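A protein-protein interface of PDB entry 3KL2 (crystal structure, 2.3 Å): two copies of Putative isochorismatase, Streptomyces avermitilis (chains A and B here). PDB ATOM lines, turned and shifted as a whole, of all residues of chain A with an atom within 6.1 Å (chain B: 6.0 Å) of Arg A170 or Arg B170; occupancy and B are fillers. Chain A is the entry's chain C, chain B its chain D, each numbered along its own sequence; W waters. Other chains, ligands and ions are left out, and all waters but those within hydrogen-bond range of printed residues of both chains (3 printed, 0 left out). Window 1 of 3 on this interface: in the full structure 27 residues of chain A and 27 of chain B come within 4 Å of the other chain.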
ATOM      1  N   ASP A 135     -18.268  26.550   7.783  1.00  0.00           N
ATOM      2  CA  ASP A 135     -17.340  27.659   7.956  1.00  0.00           C
ATOM      3  C   ASP A 135     -18.047  28.790   8.682  1.00  0.00           C
ATOM      4  O   ASP A 135     -19.054  29.270   8.209  1.00  0.00           O
ATOM      5  CB  ASP A 135     -16.895  28.146   6.557  1.00  0.00           C
ATOM      6  CG  ASP A 135     -15.885  29.280   6.616  1.00  0.00           C
ATOM      7  OD1 ASP A 135     -15.513  29.781   7.716  1.00  0.00           O
ATOM      8  OD2 ASP A 135     -15.463  29.648   5.523  1.00  0.00           O
ATOM      9  N   ASN A 162     -12.108  18.397  11.989  1.00  0.00           N
ATOM     10  CA  ASN A 162     -11.806  18.344  10.582  1.00  0.00           C
ATOM     11  C   ASN A 162     -12.938  18.902   9.744  1.00  0.00           C
ATOM     12  O   ASN A 162     -12.891  18.850   8.530  1.00  0.00           O
ATOM     13  CB  ASN A 162     -11.474  16.910  10.176  1.00  0.00           C
ATOM     14  CG  ASN A 162     -12.628  16.001  10.356  1.00  0.00           C
ATOM     15  OD1 ASN A 162     -13.344  16.084  11.356  1.00  0.00           O
ATOM     16  ND2 ASN A 162     -12.820  15.116   9.410  1.00  0.00           N
ATOM     17  N   CYS A 163     -13.958  19.459  10.379  1.00  0.00           N
ATOM     18  CA  CYS A 163     -15.086  19.987   9.609  1.00  0.00           C
ATOM     19  C   CYS A 163     -15.183  21.489   9.851  1.00  0.00           C
ATOM     20  O   CYS A 163     -14.513  22.234   9.140  1.00  0.00           O
ATOM     21  CB  CYS A 163     -16.361  19.216   9.910  1.00  0.00           C
ATOM     22  SG  CYS A 163     -17.845  19.757   9.033  1.00  0.00           S
ATOM     23  N   CYS A 164     -15.919  21.910  10.884  1.00  0.00           N
ATOM     24  CA  CYS A 164     -16.196  23.327  11.193  1.00  0.00           C
ATOM     25  C   CYS A 164     -14.965  24.108  11.702  1.00  0.00           C
ATOM     26  O   CYS A 164     -14.731  25.280  11.350  1.00  0.00           O
ATOM     27  CB  CYS A 164     -17.313  23.404  12.238  1.00  0.00           C
ATOM     28  SG  CYS A 164     -18.835  22.439  11.870  1.00  0.00           S
ATOM     29  N   VAL A 165     -14.158  23.486  12.536  1.00  0.00           N
ATOM     30  CA  VAL A 165     -12.939  24.173  12.958  1.00  0.00           C
ATOM     31  C   VAL A 165     -11.995  24.393  11.745  1.00  0.00           C
ATOM     32  O   VAL A 165     -11.545  25.511  11.484  1.00  0.00           O
ATOM     33  CB  VAL A 165     -12.257  23.434  14.140  1.00  0.00           C
ATOM     34  CG1 VAL A 165     -10.991  24.148  14.555  1.00  0.00           C
ATOM     35  CG2 VAL A 165     -13.237  23.374  15.343  1.00  0.00           C
ATOM     36  N   GLU A 166     -11.780  23.352  10.952  1.00  0.00           N
ATOM     37  CA  GLU A 166     -10.859  23.472   9.853  1.00  0.00           C
ATOM     38  C   GLU A 166     -11.363  24.462   8.768  1.00  0.00           C
ATOM     39  O   GLU A 166     -10.574  25.250   8.221  1.00  0.00           O
ATOM     40  CB  GLU A 166     -10.545  22.114   9.265  1.00  0.00           C
ATOM     41  CG  GLU A 166      -9.320  22.136   8.468  1.00  0.00           C
ATOM     42  CD  GLU A 166      -8.953  20.822   7.857  1.00  0.00           C
ATOM     43  OE1 GLU A 166      -8.788  19.837   8.590  1.00  0.00           O
ATOM     44  OE2 GLU A 166      -8.828  20.778   6.621  1.00  0.00           O
ATOM     45  N   SER A 167     -12.658  24.429   8.450  1.00  0.00           N
ATOM     46  CA  SER A 167     -13.182  25.378   7.488  1.00  0.00           C
ATOM     47  C   SER A 167     -12.929  26.787   8.003  1.00  0.00           C
ATOM     48  O   SER A 167     -12.435  27.630   7.260  1.00  0.00           O
ATOM     49  CB  SER A 167     -14.661  25.217   7.253  1.00  0.00           C
ATOM     50  OG  SER A 167     -14.871  24.100   6.458  1.00  0.00           O
ATOM     51  N   THR A 168     -13.196  27.001   9.292  1.00  0.00           N
ATOM     52  CA  THR A 168     -13.079  28.352   9.865  1.00  0.00           C
ATOM     53  C   THR A 168     -11.650  28.820   9.868  1.00  0.00           C
ATOM     54  O   THR A 168     -11.352  29.988   9.652  1.00  0.00           O
ATOM     55  CB  THR A 168     -13.634  28.398  11.269  1.00  0.00           C
ATOM     56  OG1 THR A 168     -15.028  28.009  11.233  1.00  0.00           O
ATOM     57  CG2 THR A 168     -13.503  29.809  11.880  1.00  0.00           C
ATOM     58  N   MET A 169     -10.766  27.895  10.183  1.00  0.00           N
ATOM     59  CA  MET A 169      -9.327  28.111  10.157  1.00  0.00           C
ATOM     60  C   MET A 169      -8.920  28.503   8.727  1.00  0.00           C
ATOM     61  O   MET A 169      -8.243  29.481   8.541  1.00  0.00           O
ATOM     62  CB  MET A 169      -8.625  26.818  10.597  1.00  0.00           C
ATOM     63  CG  MET A 169      -7.109  26.869  10.775  1.00  0.00           C
ATOM     64  SD  MET A 169      -6.338  25.209  10.827  1.00  0.00           S
ATOM     65  CE  MET A 169      -6.920  24.520   9.287  1.00  0.00           C
ATOM     66  N   ARG A 170      -9.376  27.758   7.736  1.00  0.00           N
ATOM     67  CA  ARG A 170      -8.978  28.007   6.315  1.00  0.00           C
ATOM     68  C   ARG A 170      -9.416  29.408   5.857  1.00  0.00           C
ATOM     69  O   ARG A 170      -8.620  30.200   5.331  1.00  0.00           O
ATOM     70  CB  ARG A 170      -9.525  26.915   5.401  1.00  0.00           C
ATOM     71  CG  ARG A 170      -8.759  25.606   5.508  1.00  0.00           C
ATOM     72  CD  ARG A 170      -9.539  24.430   4.914  1.00  0.00           C
ATOM     73  NE  ARG A 170      -8.780  23.185   5.051  1.00  0.00           N
ATOM     74  CZ  ARG A 170      -8.056  22.613   4.090  1.00  0.00           C
ATOM     75  NH1 ARG A 170      -7.948  23.145   2.871  1.00  0.00           N
ATOM     76  NH2 ARG A 170      -7.407  21.483   4.349  1.00  0.00           N
ATOM     77  N   THR A 171     -10.668  29.745   6.084  1.00  0.00           N
ATOM     78  CA  THR A 171     -11.134  31.074   5.715  1.00  0.00           C
ATOM     79  C   THR A 171     -10.391  32.163   6.543  1.00  0.00           C
ATOM     80  O   THR A 171      -9.899  33.154   5.996  1.00  0.00           O
ATOM     81  CB  THR A 171     -12.652  31.155   5.752  1.00  0.00           C
ATOM     82  OG1 THR A 171     -13.200  30.169   4.837  1.00  0.00           O
ATOM     83  CG2 THR A 171     -13.101  32.493   5.316  1.00  0.00           C
ATOM     84  N   GLY A 172     -10.231  31.986   7.831  1.00  0.00           N
ATOM     85  CA  GLY A 172      -9.469  33.002   8.598  1.00  0.00           C
ATOM     86  C   GLY A 172      -8.053  33.272   8.043  1.00  0.00           C
ATOM     87  O   GLY A 172      -7.624  34.412   7.974  1.00  0.00           O
ATOM     88  N   TYR A 173      -7.351  32.214   7.630  1.00  0.00           N
ATOM     89  CA  TYR A 173      -6.077  32.345   6.945  1.00  0.00           C
ATOM     90  C   TYR A 173      -6.196  33.197   5.684  1.00  0.00           C
ATOM     91  O   TYR A 173      -5.410  34.123   5.501  1.00  0.00           O
ATOM     92  CB  TYR A 173      -5.529  30.959   6.601  1.00  0.00           C
ATOM     93  CG  TYR A 173      -4.094  30.928   6.111  1.00  0.00           C
ATOM     94  CD1 TYR A 173      -3.057  31.112   6.976  1.00  0.00           C
ATOM     95  CD2 TYR A 173      -3.795  30.689   4.791  1.00  0.00           C
ATOM     96  CE1 TYR A 173      -1.748  31.070   6.554  1.00  0.00           C
ATOM     97  CE2 TYR A 173      -2.484  30.672   4.341  1.00  0.00           C
ATOM     98  CZ  TYR A 173      -1.448  30.870   5.243  1.00  0.00           C
ATOM     99  OH  TYR A 173      -0.100  30.822   4.854  1.00  0.00           O
ATOM    100  N   GLU A 174      -7.218  32.923   4.850  1.00  0.00           N
ATOM    101  CA  GLU A 174      -7.384  33.611   3.578  1.00  0.00           C
ATOM    102  C   GLU A 174      -7.675  35.079   3.808  1.00  0.00           C
ATOM    103  O   GLU A 174      -7.304  35.932   2.985  1.00  0.00           O
ATOM    104  CB  GLU A 174      -8.521  33.026   2.725  1.00  0.00           C
ATOM    105  CG  GLU A 174      -8.344  31.514   2.323  1.00  0.00           C
ATOM    106  CD  GLU A 174      -7.300  31.230   1.213  1.00  0.00           C
ATOM    107  OE1 GLU A 174      -6.831  32.161   0.512  1.00  0.00           O
ATOM    108  OE2 GLU A 174      -6.962  30.033   1.018  1.00  0.00           O
ATOM    109  N   ARG A 175      -8.346  35.385   4.906  1.00  0.00           N
ATOM    110  CA  ARG A 175      -8.681  36.759   5.222  1.00  0.00           C
ATOM    111  C   ARG A 175      -7.609  37.446   6.033  1.00  0.00           C
ATOM    112  O   ARG A 175      -7.823  38.504   6.488  1.00  0.00           O
ATOM    113  CB  ARG A 175     -10.055  36.809   5.921  1.00  0.00           C
ATOM    114  CG  ARG A 175     -11.115  36.119   5.037  1.00  0.00           C
ATOM    115  CD  ARG A 175     -12.547  36.397   5.400  1.00  0.00           C
ATOM    116  NE  ARG A 175     -13.473  35.658   4.512  1.00  0.00           N
ATOM    117  CZ  ARG A 175     -14.799  35.765   4.564  1.00  0.00           C
ATOM    118  NH1 ARG A 175     -15.381  36.586   5.444  1.00  0.00           N
ATOM    119  NH2 ARG A 175     -15.561  35.068   3.736  1.00  0.00           N
ATOM    120  N   ASP A 201      -3.009  19.421   8.315  1.00  0.00           N
ATOM    121  CA  ASP A 201      -3.728  20.601   7.806  1.00  0.00           C
ATOM    122  C   ASP A 201      -3.586  21.805   8.713  1.00  0.00           C
ATOM    123  O   ASP A 201      -3.496  22.931   8.218  1.00  0.00           O
ATOM    124  CB  ASP A 201      -5.213  20.288   7.587  1.00  0.00           C
ATOM    125  CG  ASP A 201      -5.450  19.181   6.560  1.00  0.00           C
ATOM    126  OD1 ASP A 201      -4.549  18.879   5.746  1.00  0.00           O
ATOM    127  OD2 ASP A 201      -6.554  18.618   6.566  1.00  0.00           O
ATOM    128  N   MET A 204      -0.671  24.174   7.972  1.00  0.00           N
ATOM    129  CA  MET A 204      -0.821  24.916   6.711  1.00  0.00           C
ATOM    130  C   MET A 204      -1.484  26.247   6.934  1.00  0.00           C
ATOM    131  O   MET A 204      -1.095  27.222   6.309  1.00  0.00           O
ATOM    132  CB  MET A 204      -1.639  24.129   5.662  1.00  0.00           C
ATOM    133  CG  MET A 204      -0.896  22.930   4.968  1.00  0.00           C
ATOM    134  SD  MET A 204      -2.034  21.912   3.947  1.00  0.00           S
ATOM    135  CE  MET A 204      -0.963  21.558   2.602  1.00  0.00           C
ATOM    136  N   PHE A 205      -2.506  26.300   7.791  1.00  0.00           N
ATOM    137  CA  PHE A 205      -3.362  27.503   7.912  1.00  0.00           C
ATOM    138  C   PHE A 205      -3.390  28.157   9.269  1.00  0.00           C
ATOM    139  O   PHE A 205      -4.192  29.072   9.481  1.00  0.00           O
ATOM    140  CB  PHE A 205      -4.792  27.206   7.549  1.00  0.00           C
ATOM    141  CG  PHE A 205      -4.977  26.545   6.184  1.00  0.00           C
ATOM    142  CD1 PHE A 205      -5.217  27.304   5.054  1.00  0.00           C
ATOM    143  CD2 PHE A 205      -4.914  25.180   6.047  1.00  0.00           C
ATOM    144  CE1 PHE A 205      -5.411  26.702   3.802  1.00  0.00           C
ATOM    145  CE2 PHE A 205      -5.102  24.580   4.813  1.00  0.00           C
ATOM    146  CZ  PHE A 205      -5.366  25.348   3.682  1.00  0.00           C
ATOM    147  N   ASN B 162      -5.331  18.015  -0.263  1.00  0.00           N
ATOM    148  CA  ASN B 162      -5.737  18.459   1.064  1.00  0.00           C
ATOM    149  C   ASN B 162      -5.562  19.976   1.363  1.00  0.00           C
ATOM    150  O   ASN B 162      -5.758  20.427   2.487  1.00  0.00           O
ATOM    151  CB  ASN B 162      -4.992  17.625   2.120  1.00  0.00           C
ATOM    152  CG  ASN B 162      -3.532  17.849   2.090  1.00  0.00           C
ATOM    153  OD1 ASN B 162      -2.945  17.964   1.019  1.00  0.00           O
ATOM    154  ND2 ASN B 162      -2.925  17.962   3.261  1.00  0.00           N
ATOM    155  N   CYS B 163      -5.230  20.765   0.352  1.00  0.00           N
ATOM    156  CA  CYS B 163      -5.002  22.160   0.545  1.00  0.00           C
ATOM    157  C   CYS B 163      -5.937  22.956  -0.360  1.00  0.00           C
ATOM    158  O   CYS B 163      -7.055  23.217   0.043  1.00  0.00           O
ATOM    159  CB  CYS B 163      -3.536  22.414   0.333  1.00  0.00           C
ATOM    160  SG  CYS B 163      -2.981  23.971   0.901  1.00  0.00           S
ATOM    161  N   CYS B 164      -5.535  23.278  -1.582  1.00  0.00           N
ATOM    162  CA  CYS B 164      -6.298  24.190  -2.399  1.00  0.00           C
ATOM    163  C   CYS B 164      -7.563  23.514  -2.911  1.00  0.00           C
ATOM    164  O   CYS B 164      -8.622  24.143  -2.943  1.00  0.00           O
ATOM    165  CB  CYS B 164      -5.436  24.741  -3.545  1.00  0.00           C
ATOM    166  SG  CYS B 164      -3.735  25.177  -3.004  1.00  0.00           S
ATOM    167  N   VAL B 165      -7.491  22.235  -3.281  1.00  0.00           N
ATOM    168  CA  VAL B 165      -8.702  21.531  -3.714  1.00  0.00           C
ATOM    169  C   VAL B 165      -9.703  21.460  -2.550  1.00  0.00           C
ATOM    170  O   VAL B 165     -10.929  21.681  -2.736  1.00  0.00           O
ATOM    171  CB  VAL B 165      -8.378  20.099  -4.227  1.00  0.00           C
ATOM    172  CG1 VAL B 165      -9.632  19.280  -4.515  1.00  0.00           C
ATOM    173  CG2 VAL B 165      -7.502  20.166  -5.481  1.00  0.00           C
ATOM    174  N   GLU B 166      -9.192  21.159  -1.359  1.00  0.00           N
ATOM    175  CA  GLU B 166     -10.059  21.065  -0.181  1.00  0.00           C
ATOM    176  C   GLU B 166     -10.689  22.424   0.226  1.00  0.00           C
ATOM    177  O   GLU B 166     -11.875  22.496   0.464  1.00  0.00           O
ATOM    178  CB  GLU B 166      -9.364  20.396   1.003  1.00  0.00           C
ATOM    179  CG  GLU B 166     -10.307  19.483   1.735  1.00  0.00           C
ATOM    180  CD  GLU B 166      -9.759  18.904   3.032  1.00  0.00           C
ATOM    181  OE1 GLU B 166      -8.936  17.950   2.997  1.00  0.00           O
ATOM    182  OE2 GLU B 166     -10.222  19.371   4.096  1.00  0.00           O
ATOM    183  N   SER B 167      -9.908  23.493   0.252  1.00  0.00           N
ATOM    184  CA  SER B 167     -10.438  24.809   0.558  1.00  0.00           C
ATOM    185  C   SER B 167     -11.496  25.199  -0.491  1.00  0.00           C
ATOM    186  O   SER B 167     -12.560  25.651  -0.145  1.00  0.00           O
ATOM    187  CB  SER B 167      -9.331  25.862   0.630  1.00  0.00           C
ATOM    188  OG  SER B 167      -8.464  25.680   1.741  1.00  0.00           O
ATOM    189  N   THR B 168     -11.221  24.994  -1.768  1.00  0.00           N
ATOM    190  CA  THR B 168     -12.135  25.426  -2.816  1.00  0.00           C
ATOM    191  C   THR B 168     -13.458  24.668  -2.717  1.00  0.00           C
ATOM    192  O   THR B 168     -14.505  25.228  -2.852  1.00  0.00           O
ATOM    193  CB  THR B 168     -11.469  25.251  -4.221  1.00  0.00           C
ATOM    194  OG1 THR B 168     -10.291  26.062  -4.246  1.00  0.00           O
ATOM    195  CG2 THR B 168     -12.388  25.661  -5.308  1.00  0.00           C
ATOM    196  N   MET B 169     -13.353  23.381  -2.449  1.00  0.00           N
ATOM    197  CA  MET B 169     -14.478  22.467  -2.240  1.00  0.00           C
ATOM    198  C   MET B 169     -15.323  22.857  -1.035  1.00  0.00           C
ATOM    199  O   MET B 169     -16.545  22.849  -1.104  1.00  0.00           O
ATOM    200  CB  MET B 169     -13.930  21.048  -2.055  1.00  0.00           C
ATOM    201  CG  MET B 169     -14.889  20.026  -1.415  1.00  0.00           C
ATOM    202  SD  MET B 169     -14.207  18.380  -1.068  1.00  0.00           S
ATOM    203  CE  MET B 169     -13.321  18.662   0.432  1.00  0.00           C
ATOM    204  N   ARG B 170     -14.679  23.172   0.069  1.00  0.00           N
ATOM    205  CA  ARG B 170     -15.419  23.612   1.253  1.00  0.00           C
ATOM    206  C   ARG B 170     -16.184  24.914   1.074  1.00  0.00           C
ATOM    207  O   ARG B 170     -17.315  25.012   1.510  1.00  0.00           O
ATOM    208  CB  ARG B 170     -14.514  23.731   2.444  1.00  0.00           C
ATOM    209  CG  ARG B 170     -14.028  22.392   2.959  1.00  0.00           C
ATOM    210  CD  ARG B 170     -12.877  22.688   3.887  1.00  0.00           C
ATOM    211  NE  ARG B 170     -12.228  21.529   4.421  1.00  0.00           N
ATOM    212  CZ  ARG B 170     -12.424  21.025   5.634  1.00  0.00           C
ATOM    213  NH1 ARG B 170     -13.314  21.546   6.479  1.00  0.00           N
ATOM    214  NH2 ARG B 170     -11.711  19.950   5.989  1.00  0.00           N
ATOM    215  N   THR B 171     -15.563  25.918   0.461  1.00  0.00           N
ATOM    216  CA  THR B 171     -16.262  27.153   0.178  1.00  0.00           C
ATOM    217  C   THR B 171     -17.338  26.888  -0.909  1.00  0.00           C
ATOM    218  O   THR B 171     -18.421  27.430  -0.849  1.00  0.00           O
ATOM    219  CB  THR B 171     -15.287  28.277  -0.140  1.00  0.00           C
ATOM    220  OG1 THR B 171     -14.298  28.380   0.908  1.00  0.00           O
ATOM    221  CG2 THR B 171     -16.015  29.641  -0.211  1.00  0.00           C
ATOM    222  N   GLY B 172     -17.093  25.976  -1.838  1.00  0.00           N
ATOM    223  CA  GLY B 172     -18.109  25.643  -2.845  1.00  0.00           C
ATOM    224  C   GLY B 172     -19.399  25.171  -2.214  1.00  0.00           C
ATOM    225  O   GLY B 172     -20.475  25.624  -2.537  1.00  0.00           O
ATOM    226  N   TYR B 173     -19.240  24.271  -1.264  1.00  0.00           N
ATOM    227  CA  TYR B 173     -20.319  23.700  -0.505  1.00  0.00           C
ATOM    228  C   TYR B 173     -21.028  24.822   0.232  1.00  0.00           C
ATOM    229  O   TYR B 173     -22.231  24.926   0.175  1.00  0.00           O
ATOM    230  CB  TYR B 173     -19.737  22.699   0.505  1.00  0.00           C
ATOM    231  CG  TYR B 173     -20.786  21.890   1.232  1.00  0.00           C
ATOM    232  CD1 TYR B 173     -21.356  20.780   0.633  1.00  0.00           C
ATOM    233  CD2 TYR B 173     -21.204  22.236   2.499  1.00  0.00           C
ATOM    234  CE1 TYR B 173     -22.328  20.033   1.271  1.00  0.00           C
ATOM    235  CE2 TYR B 173     -22.204  21.488   3.176  1.00  0.00           C
ATOM    236  CZ  TYR B 173     -22.747  20.383   2.551  1.00  0.00           C
ATOM    237  OH  TYR B 173     -23.698  19.611   3.155  1.00  0.00           O
ATOM    238  N   GLU B 174     -20.263  25.659   0.939  1.00  0.00           N
ATOM    239  CA  GLU B 174     -20.844  26.758   1.712  1.00  0.00           C
ATOM    240  C   GLU B 174     -21.751  27.629   0.844  1.00  0.00           C
ATOM    241  O   GLU B 174     -22.754  28.140   1.309  1.00  0.00           O
ATOM    242  CB  GLU B 174     -19.758  27.662   2.267  1.00  0.00           C
ATOM    243  CG  GLU B 174     -18.980  27.120   3.399  1.00  0.00           C
ATOM    244  CD  GLU B 174     -19.878  26.657   4.584  1.00  0.00           C
ATOM    245  OE1 GLU B 174     -20.907  27.294   4.872  1.00  0.00           O
ATOM    246  OE2 GLU B 174     -19.514  25.680   5.241  1.00  0.00           O
ATOM    247  N   ARG B 175     -21.351  27.799  -0.413  1.00  0.00           N
ATOM    248  CA  ARG B 175     -22.030  28.653  -1.355  1.00  0.00           C
ATOM    249  C   ARG B 175     -23.072  27.949  -2.160  1.00  0.00           C
ATOM    250  O   ARG B 175     -23.691  28.548  -2.970  1.00  0.00           O
ATOM    251  CB  ARG B 175     -21.012  29.379  -2.241  1.00  0.00           C
ATOM    252  CG  ARG B 175     -20.315  30.443  -1.396  1.00  0.00           C
ATOM    253  CD  ARG B 175     -19.273  31.207  -2.116  1.00  0.00           C
ATOM    254  NE  ARG B 175     -18.300  31.816  -1.203  1.00  0.00           N
ATOM    255  CZ  ARG B 175     -17.432  32.751  -1.563  1.00  0.00           C
ATOM    256  NH1 ARG B 175     -17.437  33.216  -2.802  1.00  0.00           N
ATOM    257  NH2 ARG B 175     -16.556  33.234  -0.695  1.00  0.00           N
ATOM    258  N   ASP B 201     -12.773  13.752   4.344  1.00  0.00           N
ATOM    259  CA  ASP B 201     -13.289  15.129   4.232  1.00  0.00           C
ATOM    260  C   ASP B 201     -14.115  15.331   2.967  1.00  0.00           C
ATOM    261  O   ASP B 201     -15.115  16.029   2.986  1.00  0.00           O
ATOM    262  CB  ASP B 201     -12.171  16.154   4.280  1.00  0.00           C
ATOM    263  CG  ASP B 201     -11.331  16.100   5.557  1.00  0.00           C
ATOM    264  OD1 ASP B 201     -11.752  15.549   6.593  1.00  0.00           O
ATOM    265  OD2 ASP B 201     -10.196  16.630   5.519  1.00  0.00           O
ATOM    266  N   MET B 204     -17.928  14.970   3.109  1.00  0.00           N
ATOM    267  CA  MET B 204     -18.630  15.939   3.924  1.00  0.00           C
ATOM    268  C   MET B 204     -19.034  17.102   3.016  1.00  0.00           C
ATOM    269  O   MET B 204     -20.105  17.666   3.180  1.00  0.00           O
ATOM    270  CB  MET B 204     -17.723  16.450   5.080  1.00  0.00           C
ATOM    271  CG  MET B 204     -17.515  15.574   6.378  1.00  0.00           C
ATOM    272  SD  MET B 204     -16.164  16.304   7.436  1.00  0.00           S
ATOM    273  CE  MET B 204     -16.895  16.232   9.004  1.00  0.00           C
ATOM    274  N   PHE B 205     -18.202  17.443   2.034  1.00  0.00           N
ATOM    275  CA  PHE B 205     -18.384  18.695   1.262  1.00  0.00           C
ATOM    276  C   PHE B 205     -18.625  18.497  -0.249  1.00  0.00           C
ATOM    277  O   PHE B 205     -18.782  19.477  -1.003  1.00  0.00           O
ATOM    278  CB  PHE B 205     -17.188  19.618   1.485  1.00  0.00           C
ATOM    279  CG  PHE B 205     -16.969  20.010   2.931  1.00  0.00           C
ATOM    280  CD1 PHE B 205     -17.627  21.105   3.479  1.00  0.00           C
ATOM    281  CD2 PHE B 205     -16.111  19.310   3.732  1.00  0.00           C
ATOM    282  CE1 PHE B 205     -17.419  21.485   4.781  1.00  0.00           C
ATOM    283  CE2 PHE B 205     -15.902  19.681   5.044  1.00  0.00           C
ATOM    284  CZ  PHE B 205     -16.561  20.766   5.573  1.00  0.00           C
HETATM  285  O   HOH W   1     -21.233  28.655   6.937  1.00  0.00           O
HETATM  286  O   HOH W   2     -16.656  25.073   4.914  1.00  0.00           O
HETATM  287  O   HOH W   3      -8.379  28.247   2.419  1.00  0.00           O
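Hydrophobic or aromatic side chains of chain A that line the printed part of chain B: Met A204 and Phe A205. Of the 17 printed residues of chain B, 9 touch a printed residue of chain A. Printed residues of chain B that touch a printed residue of chain A: Asn B162, Cys B163, Glu B166, Ser B167, Arg B170, Glu B174, Asp B201, Met B204 and Phe B205. Hydrophobic or aromatic side chains of chain B that line the printed part of chain A: Met B204 and Phe B205. Along chain B the printed residues that touch a printed residue of chain A span positions 162 to 205.
Asn A162 touches Asp B201, and with the chains exchanged Asp A201 touches Asn B162. Cys A163 touches Arg B170, and with the chains exchanged Arg A170 touches Cys B163. Cys A163 touches Phe B205, and with the chains exchanged Phe A205 touches Cys B163. Glu A166 touches Arg B170, and with the chains exchanged Arg A170 touches Glu B166. 17 positions are printed for both chains.
The guanidinium group (NH2) of Arg A170 is in salt-bridge range of the side-chain carboxylate (OD2) of Asp A201, at 3.7 Å. OE2 of Glu B166 lies within salt-bridge range of NH2 of Arg B170 (2.5 Å). OG1 of Thr B171 is in hydrogen-bond range of O of Ser B167 (3.4 Å). The guanidinium group of Arg B170 is in salt-bridge range of the side-chain carboxylate of Asp B201, at 3.7 Å. The guanidinium group of Arg A170 is in salt-bridge range of the side-chain carboxylate of Glu A166, 2.8 Å away. OG1 of Thr A171 sits at hydrogen-bond distance from OD2 of Asp A135.
The side-chain sulfur (SD) of Met A204 sits close to the side-chain sulfur (SG) of Cys B163, at 3.8 Å. The side-chain amide nitrogen (ND2) of Asn A162 is in hydrogen-bond range of the side-chain carboxylate (OD1) of Asp B201 (3.0 Å). OD1 of Asp A201 lies within hydrogen-bond range of ND2 of Asn B162, 3.1 Å away. NH2 of Arg A170 lies within hydrogen-bond range of O of Asn B162, at 2.7 Å. NH1 of Arg A170 lies within hydrogen-bond range of OG of Ser B167 (2.8 Å). OE2 of Glu B166 lies within salt-bridge range of NH2 of Arg A170 (3.5 Å). The guanidinium group (NH2) of Arg B170 is in hydrogen-bond range of the backbone carbonyl oxygen (O) of Asn A162, 3.0 Å away. N of Asp A135 sits at hydrogen-bond distance from OE2 of Glu B174 (3.0 Å). OE2 of Glu A166 is in salt-bridge range of NH2 of Arg B170. The side-chain carboxylate (OE2) of Glu B166 sits close to the side-chain carboxylate (OE2) of Glu A166 (3.2 Å). NH1 of Arg B170 lies within hydrogen-bond range of OG of Ser A167 (3.0 Å). The backbone carbonyl oxygen of Cys A163 sits at hydrogen-bond distance from the guanidinium group of Arg B170. NH1 of Arg A170 lies within hydrogen-bond range of O of Cys B163 (3.0 Å).
Met B204 touches Cys A163. Cys A163 touches Phe B205 (SG to CZ, 3.8 Å). OG of Ser A167 touches CZ of Phe B205, 3.8 Å away. Arg A170 touches Arg B170 (NE to NE, 3.9 Å). Phe A205 touches Cys B163. Ser B167 touches Phe A205.
Water W1 lies within hydrogen-bond range of OE1 of Glu B174 (2.5 Å) and O of Asp A135 (2.6 Å). Water W2 lies within hydrogen-bond range of the side-chain hydroxyl of Ser A167 (2.6 Å), the side-chain carboxylate of Glu B174 (2.9 Å) and the backbone carbonyl oxygen of Arg B170 (3.5 Å). Water W3 lies within hydrogen-bond range of the side-chain hydroxyl (OG) of Ser B167 (2.7 Å) and the side-chain carboxylate (OE2) of Glu A174 (2.7 Å).
Of chain B, only Asn B162, Cys B163, Glu B166, Ser B167 and Arg B170 come within 4 Å of Arg A170. Thr A171 touches none of the printed residues of chain B. Printed residues of chain B within 4 Å of Phe A205: Cys B163 and Ser B167. Printed residues of chain A within 4 Å of Asn B162: Arg A170 and Asp A201. Printed residues of chain A within 4 Å of Ser B167: Arg A170 and Phe A205. Met B169 touches none of the printed residues of chain A. Of chain A, only Asn A162, Cys A163, Glu A166, Ser A167 and Arg A170 come within 4 Å of Arg B170. The nearest residue of chain B that does not touch Arg A170 is Cys B164 (5.1 Å). The nearest printed residue of chain A that does not touch Asn B162 is Met A204 (4.1 Å).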
